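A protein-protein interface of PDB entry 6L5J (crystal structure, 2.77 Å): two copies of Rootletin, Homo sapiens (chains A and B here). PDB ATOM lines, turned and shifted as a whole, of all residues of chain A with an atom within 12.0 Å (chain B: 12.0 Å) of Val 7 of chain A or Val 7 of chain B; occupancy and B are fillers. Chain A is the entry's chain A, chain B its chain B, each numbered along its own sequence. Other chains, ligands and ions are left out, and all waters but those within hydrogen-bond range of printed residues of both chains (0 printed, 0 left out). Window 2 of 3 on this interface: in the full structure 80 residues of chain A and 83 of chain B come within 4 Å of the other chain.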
ATOM      1  N   MET A   3      29.901  -8.393  10.849  1.00  0.00           N
ATOM      2  CA  MET A   3      30.674  -7.288  11.410  1.00  0.00           C
ATOM      3  C   MET A   3      30.990  -7.490  12.879  1.00  0.00           C
ATOM      4  O   MET A   3      30.693  -8.534  13.457  1.00  0.00           O
ATOM      5  CB  MET A   3      29.927  -5.964  11.252  1.00  0.00           C
ATOM      6  CG  MET A   3      29.836  -5.455   9.832  1.00  0.00           C
ATOM      7  SD  MET A   3      28.812  -3.800   9.737  1.00  0.00           S
ATOM      8  CE  MET A   3      30.122  -2.532  10.435  1.00  0.00           C
ATOM      9  N   GLU A   4      31.594  -6.464  13.475  1.00  0.00           N
ATOM     10  CA  GLU A   4      31.926  -6.501  14.891  1.00  0.00           C
ATOM     11  C   GLU A   4      31.445  -5.250  15.615  1.00  0.00           C
ATOM     12  O   GLU A   4      31.071  -5.321  16.790  1.00  0.00           O
ATOM     13  CB  GLU A   4      33.433  -6.670  15.090  1.00  0.00           C
ATOM     14  CG  GLU A   4      33.959  -8.050  14.751  1.00  0.00           C
ATOM     15  CD  GLU A   4      35.450  -8.171  14.998  1.00  0.00           C
ATOM     16  OE1 GLU A   4      36.091  -7.146  15.311  1.00  0.00           O
ATOM     17  OE2 GLU A   4      35.990  -9.291  14.873  1.00  0.00           O
ATOM     18  N   SER A   5      31.452  -4.102  14.930  1.00  0.00           N
ATOM     19  CA  SER A   5      31.069  -2.852  15.580  1.00  0.00           C
ATOM     20  C   SER A   5      29.601  -2.870  15.991  1.00  0.00           C
ATOM     21  O   SER A   5      29.255  -2.520  17.127  1.00  0.00           O
ATOM     22  CB  SER A   5      31.355  -1.672  14.653  1.00  0.00           C
ATOM     23  OG  SER A   5      30.574  -1.760  13.477  1.00  0.00           O
ATOM     24  N   THR A   6      28.722  -3.279  15.080  1.00  0.00           N
ATOM     25  CA  THR A   6      27.309  -3.324  15.419  1.00  0.00           C
ATOM     26  C   THR A   6      26.967  -4.533  16.282  1.00  0.00           C
ATOM     27  O   THR A   6      26.004  -4.475  17.052  1.00  0.00           O
ATOM     28  CB  THR A   6      26.459  -3.322  14.147  1.00  0.00           C
ATOM     29  OG1 THR A   6      26.736  -4.502  13.384  1.00  0.00           O
ATOM     30  CG2 THR A   6      26.763  -2.084  13.305  1.00  0.00           C
ATOM     31  N   VAL A   7      27.739  -5.621  16.196  1.00  0.00           N
ATOM     32  CA  VAL A   7      27.396  -6.817  16.964  1.00  0.00           C
ATOM     33  C   VAL A   7      27.626  -6.589  18.459  1.00  0.00           C
ATOM     34  O   VAL A   7      26.899  -7.135  19.300  1.00  0.00           O
ATOM     35  CB  VAL A   7      28.169  -8.036  16.428  1.00  0.00           C
ATOM     36  CG1 VAL A   7      27.909  -9.270  17.277  1.00  0.00           C
ATOM     37  CG2 VAL A   7      27.758  -8.312  15.003  1.00  0.00           C
ATOM     38  N   ASN A   8      28.610  -5.755  18.823  1.00  0.00           N
ATOM     39  CA  ASN A   8      28.874  -5.506  20.243  1.00  0.00           C
ATOM     40  C   ASN A   8      27.892  -4.498  20.843  1.00  0.00           C
ATOM     41  O   ASN A   8      27.516  -4.617  22.017  1.00  0.00           O
ATOM     42  CB  ASN A   8      30.313  -5.024  20.452  1.00  0.00           C
ATOM     43  CG  ASN A   8      31.346  -6.112  20.196  1.00  0.00           C
ATOM     44  OD1 ASN A   8      32.147  -6.018  19.262  1.00  0.00           O
ATOM     45  ND2 ASN A   8      31.340  -7.146  21.038  1.00  0.00           N
ATOM     46  N   ALA A   9      27.493  -3.479  20.075  1.00  0.00           N
ATOM     47  CA  ALA A   9      26.500  -2.537  20.581  1.00  0.00           C
ATOM     48  C   ALA A   9      25.161  -3.227  20.796  1.00  0.00           C
ATOM     49  O   ALA A   9      24.429  -2.897  21.736  1.00  0.00           O
ATOM     50  CB  ALA A   9      26.355  -1.349  19.630  1.00  0.00           C
ATOM     51  N   LEU A  10      24.832  -4.206  19.949  1.00  0.00           N
ATOM     52  CA  LEU A  10      23.602  -4.950  20.181  1.00  0.00           C
ATOM     53  C   LEU A  10      23.779  -5.987  21.291  1.00  0.00           C
ATOM     54  O   LEU A  10      22.878  -6.153  22.118  1.00  0.00           O
ATOM     55  CB  LEU A  10      23.111  -5.600  18.884  1.00  0.00           C
ATOM     56  CG  LEU A  10      22.732  -4.692  17.701  1.00  0.00           C
ATOM     57  CD1 LEU A  10      22.217  -5.551  16.565  1.00  0.00           C
ATOM     58  CD2 LEU A  10      21.730  -3.582  18.029  1.00  0.00           C
ATOM     59  N   THR A  11      24.925  -6.681  21.354  1.00  0.00           N
ATOM     60  CA  THR A  11      25.150  -7.582  22.485  1.00  0.00           C
ATOM     61  C   THR A  11      25.181  -6.807  23.798  1.00  0.00           C
ATOM     62  O   THR A  11      24.797  -7.341  24.845  1.00  0.00           O
ATOM     63  CB  THR A  11      26.444  -8.387  22.303  1.00  0.00           C
ATOM     64  OG1 THR A  11      26.375  -9.142  21.090  1.00  0.00           O
ATOM     65  CG2 THR A  11      26.634  -9.373  23.456  1.00  0.00           C
ATOM     66  N   SER A  12      25.607  -5.537  23.755  1.00  0.00           N
ATOM     67  CA  SER A  12      25.488  -4.666  24.923  1.00  0.00           C
ATOM     68  C   SER A  12      24.028  -4.406  25.285  1.00  0.00           C
ATOM     69  O   SER A  12      23.709  -4.218  26.464  1.00  0.00           O
ATOM     70  CB  SER A  12      26.218  -3.344  24.667  1.00  0.00           C
ATOM     71  OG  SER A  12      26.085  -2.449  25.761  1.00  0.00           O
ATOM     72  N   GLU A  13      23.137  -4.376  24.288  1.00  0.00           N
ATOM     73  CA  GLU A  13      21.708  -4.253  24.561  1.00  0.00           C
ATOM     74  C   GLU A  13      21.156  -5.538  25.168  1.00  0.00           C
ATOM     75  O   GLU A  13      20.355  -5.493  26.112  1.00  0.00           O
ATOM     76  CB  GLU A  13      20.956  -3.898  23.275  1.00  0.00           C
ATOM     77  CG  GLU A  13      21.229  -2.494  22.754  1.00  0.00           C
ATOM     78  CD  GLU A  13      20.637  -1.416  23.642  1.00  0.00           C
ATOM     79  OE1 GLU A  13      19.549  -1.648  24.221  1.00  0.00           O
ATOM     80  OE2 GLU A  13      21.268  -0.345  23.767  1.00  0.00           O
ATOM     81  N   LEU A  14      21.568  -6.689  24.627  1.00  0.00           N
ATOM     82  CA  LEU A  14      21.232  -7.978  25.226  1.00  0.00           C
ATOM     83  C   LEU A  14      21.641  -8.035  26.691  1.00  0.00           C
ATOM     84  O   LEU A  14      20.878  -8.506  27.541  1.00  0.00           O
ATOM     85  CB  LEU A  14      21.900  -9.104  24.433  1.00  0.00           C
ATOM     86  CG  LEU A  14      21.729 -10.572  24.834  1.00  0.00           C
ATOM     87  CD1 LEU A  14      21.792 -11.480  23.604  1.00  0.00           C
ATOM     88  CD2 LEU A  14      22.800 -10.980  25.842  1.00  0.00           C
ATOM     89  N   ARG A  15      22.851  -7.575  27.007  1.00  0.00           N
ATOM     90  CA  ARG A  15      23.279  -7.559  28.400  1.00  0.00           C
ATOM     91  C   ARG A  15      22.520  -6.523  29.215  1.00  0.00           C
ATOM     92  O   ARG A  15      22.277  -6.735  30.409  1.00  0.00           O
ATOM     93  CB  ARG A  15      24.774  -7.295  28.476  1.00  0.00           C
ATOM     94  CG  ARG A  15      25.366  -7.257  29.866  1.00  0.00           C
ATOM     95  CD  ARG A  15      26.834  -7.047  29.685  1.00  0.00           C
ATOM     96  NE  ARG A  15      27.130  -5.742  29.095  1.00  0.00           N
ATOM     97  CZ  ARG A  15      28.236  -5.470  28.403  1.00  0.00           C
ATOM     98  NH1 ARG A  15      29.124  -6.432  28.177  1.00  0.00           N
ATOM     99  NH2 ARG A  15      28.436  -4.253  27.904  1.00  0.00           N
ATOM    100  N   ASP A  16      22.133  -5.406  28.595  1.00  0.00           N
ATOM    101  CA  ASP A  16      21.540  -4.309  29.353  1.00  0.00           C
ATOM    102  C   ASP A  16      20.129  -4.659  29.818  1.00  0.00           C
ATOM    103  O   ASP A  16      19.781  -4.433  30.979  1.00  0.00           O
ATOM    104  CB  ASP A  16      21.572  -3.023  28.514  1.00  0.00           C
ATOM    105  CG  ASP A  16      21.187  -1.780  29.307  1.00  0.00           C
ATOM    106  OD1 ASP A  16      20.630  -1.910  30.416  1.00  0.00           O
ATOM    107  OD2 ASP A  16      21.493  -0.664  28.836  1.00  0.00           O
ATOM    108  N   GLU B   4      25.545 -11.513   9.296  1.00  0.00           N
ATOM    109  CA  GLU B   4      24.197 -11.737   8.788  1.00  0.00           C
ATOM    110  C   GLU B   4      23.429 -12.692   9.698  1.00  0.00           C
ATOM    111  O   GLU B   4      22.464 -12.288  10.344  1.00  0.00           O
ATOM    112  CB  GLU B   4      24.232 -12.292   7.358  1.00  0.00           C
ATOM    113  CG  GLU B   4      24.763 -11.321   6.296  1.00  0.00           C
ATOM    114  CD  GLU B   4      26.284 -11.332   6.157  1.00  0.00           C
ATOM    115  OE1 GLU B   4      26.952 -12.146   6.832  1.00  0.00           O
ATOM    116  OE2 GLU B   4      26.814 -10.522   5.367  1.00  0.00           O
ATOM    117  N   SER B   5      23.862 -13.960   9.739  1.00  0.00           N
ATOM    118  CA  SER B   5      23.211 -14.957  10.588  1.00  0.00           C
ATOM    119  C   SER B   5      23.508 -14.735  12.065  1.00  0.00           C
ATOM    120  O   SER B   5      22.770 -15.245  12.918  1.00  0.00           O
ATOM    121  CB  SER B   5      23.632 -16.376  10.183  1.00  0.00           C
ATOM    122  OG  SER B   5      24.985 -16.624  10.520  1.00  0.00           O
ATOM    123  N   THR B   6      24.572 -13.993  12.382  1.00  0.00           N
ATOM    124  CA  THR B   6      24.850 -13.621  13.764  1.00  0.00           C
ATOM    125  C   THR B   6      24.011 -12.429  14.195  1.00  0.00           C
ATOM    126  O   THR B   6      23.476 -12.418  15.309  1.00  0.00           O
ATOM    127  CB  THR B   6      26.338 -13.314  13.947  1.00  0.00           C
ATOM    128  OG1 THR B   6      27.095 -14.509  13.732  1.00  0.00           O
ATOM    129  CG2 THR B   6      26.631 -12.783  15.340  1.00  0.00           C
ATOM    130  N   VAL B   7      23.863 -11.427  13.330  1.00  0.00           N
ATOM    131  CA  VAL B   7      23.198 -10.206  13.771  1.00  0.00           C
ATOM    132  C   VAL B   7      21.682 -10.398  13.796  1.00  0.00           C
ATOM    133  O   VAL B   7      20.998  -9.898  14.697  1.00  0.00           O
ATOM    134  CB  VAL B   7      23.622  -9.019  12.888  1.00  0.00           C
ATOM    135  CG1 VAL B   7      23.117  -7.702  13.482  1.00  0.00           C
ATOM    136  CG2 VAL B   7      25.135  -8.997  12.714  1.00  0.00           C
ATOM    137  N   ASN B   8      21.127 -11.147  12.834  1.00  0.00           N
ATOM    138  CA  ASN B   8      19.675 -11.327  12.804  1.00  0.00           C
ATOM    139  C   ASN B   8      19.193 -12.234  13.940  1.00  0.00           C
ATOM    140  O   ASN B   8      18.125 -11.987  14.517  1.00  0.00           O
ATOM    141  CB  ASN B   8      19.240 -11.896  11.450  1.00  0.00           C
ATOM    142  CG  ASN B   8      17.736 -11.739  11.194  1.00  0.00           C
ATOM    143  OD1 ASN B   8      17.015 -11.129  11.988  1.00  0.00           O
ATOM    144  ND2 ASN B   8      17.261 -12.307  10.084  1.00  0.00           N
ATOM    145  N   ALA B   9      19.959 -13.284  14.269  1.00  0.00           N
ATOM    146  CA  ALA B   9      19.576 -14.200  15.344  1.00  0.00           C
ATOM    147  C   ALA B   9      19.557 -13.506  16.699  1.00  0.00           C
ATOM    148  O   ALA B   9      18.749 -13.858  17.571  1.00  0.00           O
ATOM    149  CB  ALA B   9      20.534 -15.389  15.379  1.00  0.00           C
ATOM    150  N   LEU B  10      20.439 -12.522  16.890  1.00  0.00           N
ATOM    151  CA  LEU B  10      20.464 -11.765  18.134  1.00  0.00           C
ATOM    152  C   LEU B  10      19.366 -10.705  18.157  1.00  0.00           C
ATOM    153  O   LEU B  10      18.712 -10.524  19.186  1.00  0.00           O
ATOM    154  CB  LEU B  10      21.848 -11.135  18.333  1.00  0.00           C
ATOM    155  CG  LEU B  10      23.048 -12.093  18.430  1.00  0.00           C
ATOM    156  CD1 LEU B  10      24.366 -11.330  18.564  1.00  0.00           C
ATOM    157  CD2 LEU B  10      22.896 -13.116  19.551  1.00  0.00           C
ATOM    158  N   THR B  11      19.138 -10.009  17.034  1.00  0.00           N
ATOM    159  CA  THR B  11      18.071  -9.010  16.975  1.00  0.00           C
ATOM    160  C   THR B  11      16.700  -9.638  17.204  1.00  0.00           C
ATOM    161  O   THR B  11      15.805  -8.984  17.755  1.00  0.00           O
ATOM    162  CB  THR B  11      18.102  -8.270  15.634  1.00  0.00           C
ATOM    163  OG1 THR B  11      19.349  -7.589  15.501  1.00  0.00           O
ATOM    164  CG2 THR B  11      16.981  -7.230  15.547  1.00  0.00           C
ATOM    165  N   SER B  12      16.518 -10.899  16.807  1.00  0.00           N
ATOM    166  CA  SER B  12      15.262 -11.585  17.099  1.00  0.00           C
ATOM    167  C   SER B  12      15.030 -11.704  18.606  1.00  0.00           C
ATOM    168  O   SER B  12      13.900 -11.539  19.087  1.00  0.00           O
ATOM    169  CB  SER B  12      15.251 -12.961  16.426  1.00  0.00           C
ATOM    170  OG  SER B  12      16.292 -13.790  16.914  1.00  0.00           O
ATOM    171  N   GLU B  13      16.093 -11.971  19.372  1.00  0.00           N
ATOM    172  CA  GLU B  13      15.950 -12.073  20.820  1.00  0.00           C
ATOM    173  C   GLU B  13      15.844 -10.698  21.467  1.00  0.00           C
ATOM    174  O   GLU B  13      15.185 -10.558  22.503  1.00  0.00           O
ATOM    175  CB  GLU B  13      17.122 -12.861  21.412  1.00  0.00           C
ATOM    176  CG  GLU B  13      17.203 -14.298  20.920  1.00  0.00           C
ATOM    177  CD  GLU B  13      16.000 -15.127  21.326  1.00  0.00           C
ATOM    178  OE1 GLU B  13      15.442 -14.874  22.410  1.00  0.00           O
ATOM    179  OE2 GLU B  13      15.600 -16.025  20.556  1.00  0.00           O
ATOM    180  N   LEU B  14      16.472  -9.679  20.872  1.00  0.00           N
ATOM    181  CA  LEU B  14      16.361  -8.322  21.400  1.00  0.00           C
ATOM    182  C   LEU B  14      14.959  -7.773  21.219  1.00  0.00           C
ATOM    183  O   LEU B  14      14.473  -7.008  22.057  1.00  0.00           O
ATOM    184  CB  LEU B  14      17.357  -7.386  20.723  1.00  0.00           C
ATOM    185  CG  LEU B  14      17.313  -5.940  21.239  1.00  0.00           C
ATOM    186  CD1 LEU B  14      17.820  -5.874  22.665  1.00  0.00           C
ATOM    187  CD2 LEU B  14      18.060  -4.949  20.351  1.00  0.00           C
ATOM    188  N   ARG B  15      14.297  -8.116  20.117  1.00  0.00           N
ATOM    189  CA  ARG B  15      12.889  -7.754  20.013  1.00  0.00           C
ATOM    190  C   ARG B  15      12.042  -8.621  20.935  1.00  0.00           C
ATOM    191  O   ARG B  15      11.007  -8.171  21.441  1.00  0.00           O
ATOM    192  CB  ARG B  15      12.423  -7.890  18.568  1.00  0.00           C
ATOM    193  CG  ARG B  15      11.055  -7.300  18.286  1.00  0.00           C
ATOM    194  CD  ARG B  15      10.687  -7.593  16.850  1.00  0.00           C
ATOM    195  NE  ARG B  15      10.557  -9.035  16.664  1.00  0.00           N
ATOM    196  CZ  ARG B  15      11.384  -9.788  15.943  1.00  0.00           C
ATOM    197  NH1 ARG B  15      12.423  -9.245  15.323  1.00  0.00           N
ATOM    198  NH2 ARG B  15      11.172 -11.095  15.845  1.00  0.00           N
ATOM    199  N   ASP B  16      12.489  -9.858  21.174  1.00  0.00           N
ATOM    200  CA  ASP B  16      11.757 -10.790  22.023  1.00  0.00           C
ATOM    201  C   ASP B  16      11.738 -10.317  23.474  1.00  0.00           C
ATOM    202  O   ASP B  16      10.693 -10.363  24.138  1.00  0.00           O
ATOM    203  CB  ASP B  16      12.385 -12.181  21.896  1.00  0.00           C
ATOM    204  CG  ASP B  16      11.532 -13.269  22.498  1.00  0.00           C
ATOM    205  OD1 ASP B  16      10.469 -12.948  23.060  1.00  0.00           O
ATOM    206  OD2 ASP B  16      11.916 -14.446  22.399  1.00  0.00           O
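Among the printed residues, pairs that only touch across the chains: Val 7 of chain A with Val 7 of chain B (3.5 Å), Leu 10 of chain A with Thr 11 of chain B (3.7 Å), Glu 13 of chain A with Leu 14 of chain B (3.8 Å), Leu 10 of chain A with Val 7 of chain B (3.9 Å) and Thr 11 of chain A with Leu 10 of chain B (3.9 Å).
Of the 14 printed residues of chain A, 4 touch a printed residue of chain B. Hydrophobic or aromatic side chains of chain B that line the printed part of chain A: Val 7, Leu 10 and Leu 14. Among the printed residues, 5 pairs touch across the chains. Among the printed residues, no Asp or Glu carboxylate lies within 4 Å of a Lys or Arg side-chain nitrogen of the other chain.
Val 7 of chain A touches its own counterpart, Val 7 of chain B. Leu 10 of chain A touches Val 7 of chain B, but with the chains exchanged Val 7 of chain A does not touch Leu 10 of chain B (4.3 Å). Leu 10 of chain A touches Thr 11 of chain B, and with the chains exchanged Thr 11 of chain A touches Leu 10 of chain B. Glu 13 of chain A touches Leu 14 of chain B, but with the chains exchanged Leu 14 of chain A does not touch Glu 13 of chain B (5.3 Å). 13 positions are printed for both chains.
The backbone carbonyl oxygen (O) of Val 7 of chain A is in hydrogen-bond range of the side-chain hydroxyl (OG1) of Thr 11 of chain A (2.7 Å). O of Val 7 of chain B is in hydrogen-bond range of OG1 of Thr 11 of chain B.
Val 7 of chain A touches one residue of chain B. Of chain A, only Val 7 and Leu 10 come within 4 Å of Val 7 of chain B. No residue of chain B comes within 4 Å of Ser 5 of chain A. No residue of chain B comes within 4 Å of Thr 6 of chain A. No residue of chain B comes within 4 Å of Asn 8 of chain A. No residue of chain B comes within 4 Å of Ala 9 of chain A. Of chain B, only Leu 10 (3.9 Å) comes within 4 Å of Thr 11 of chain A. No residue of chain A comes within 4 Å of Glu 4 of chain B. Ser 5 of chain B touches none of the printed residues of chain A. No residue of chain A comes within 4 Å of Asn 8 of chain B. Of chain A, only Thr 11 (3.9 Å) comes within 4 Å of Leu 10 of chain B. Thr 11 of chain B touches just one residue of chain A: Leu 10 (3.7 Å). Of the printed residues of chain B, Glu 13 of chain A touches Leu 14. Printed residues of chain A within 4 Å of Leu 14 of chain B: Glu 13.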
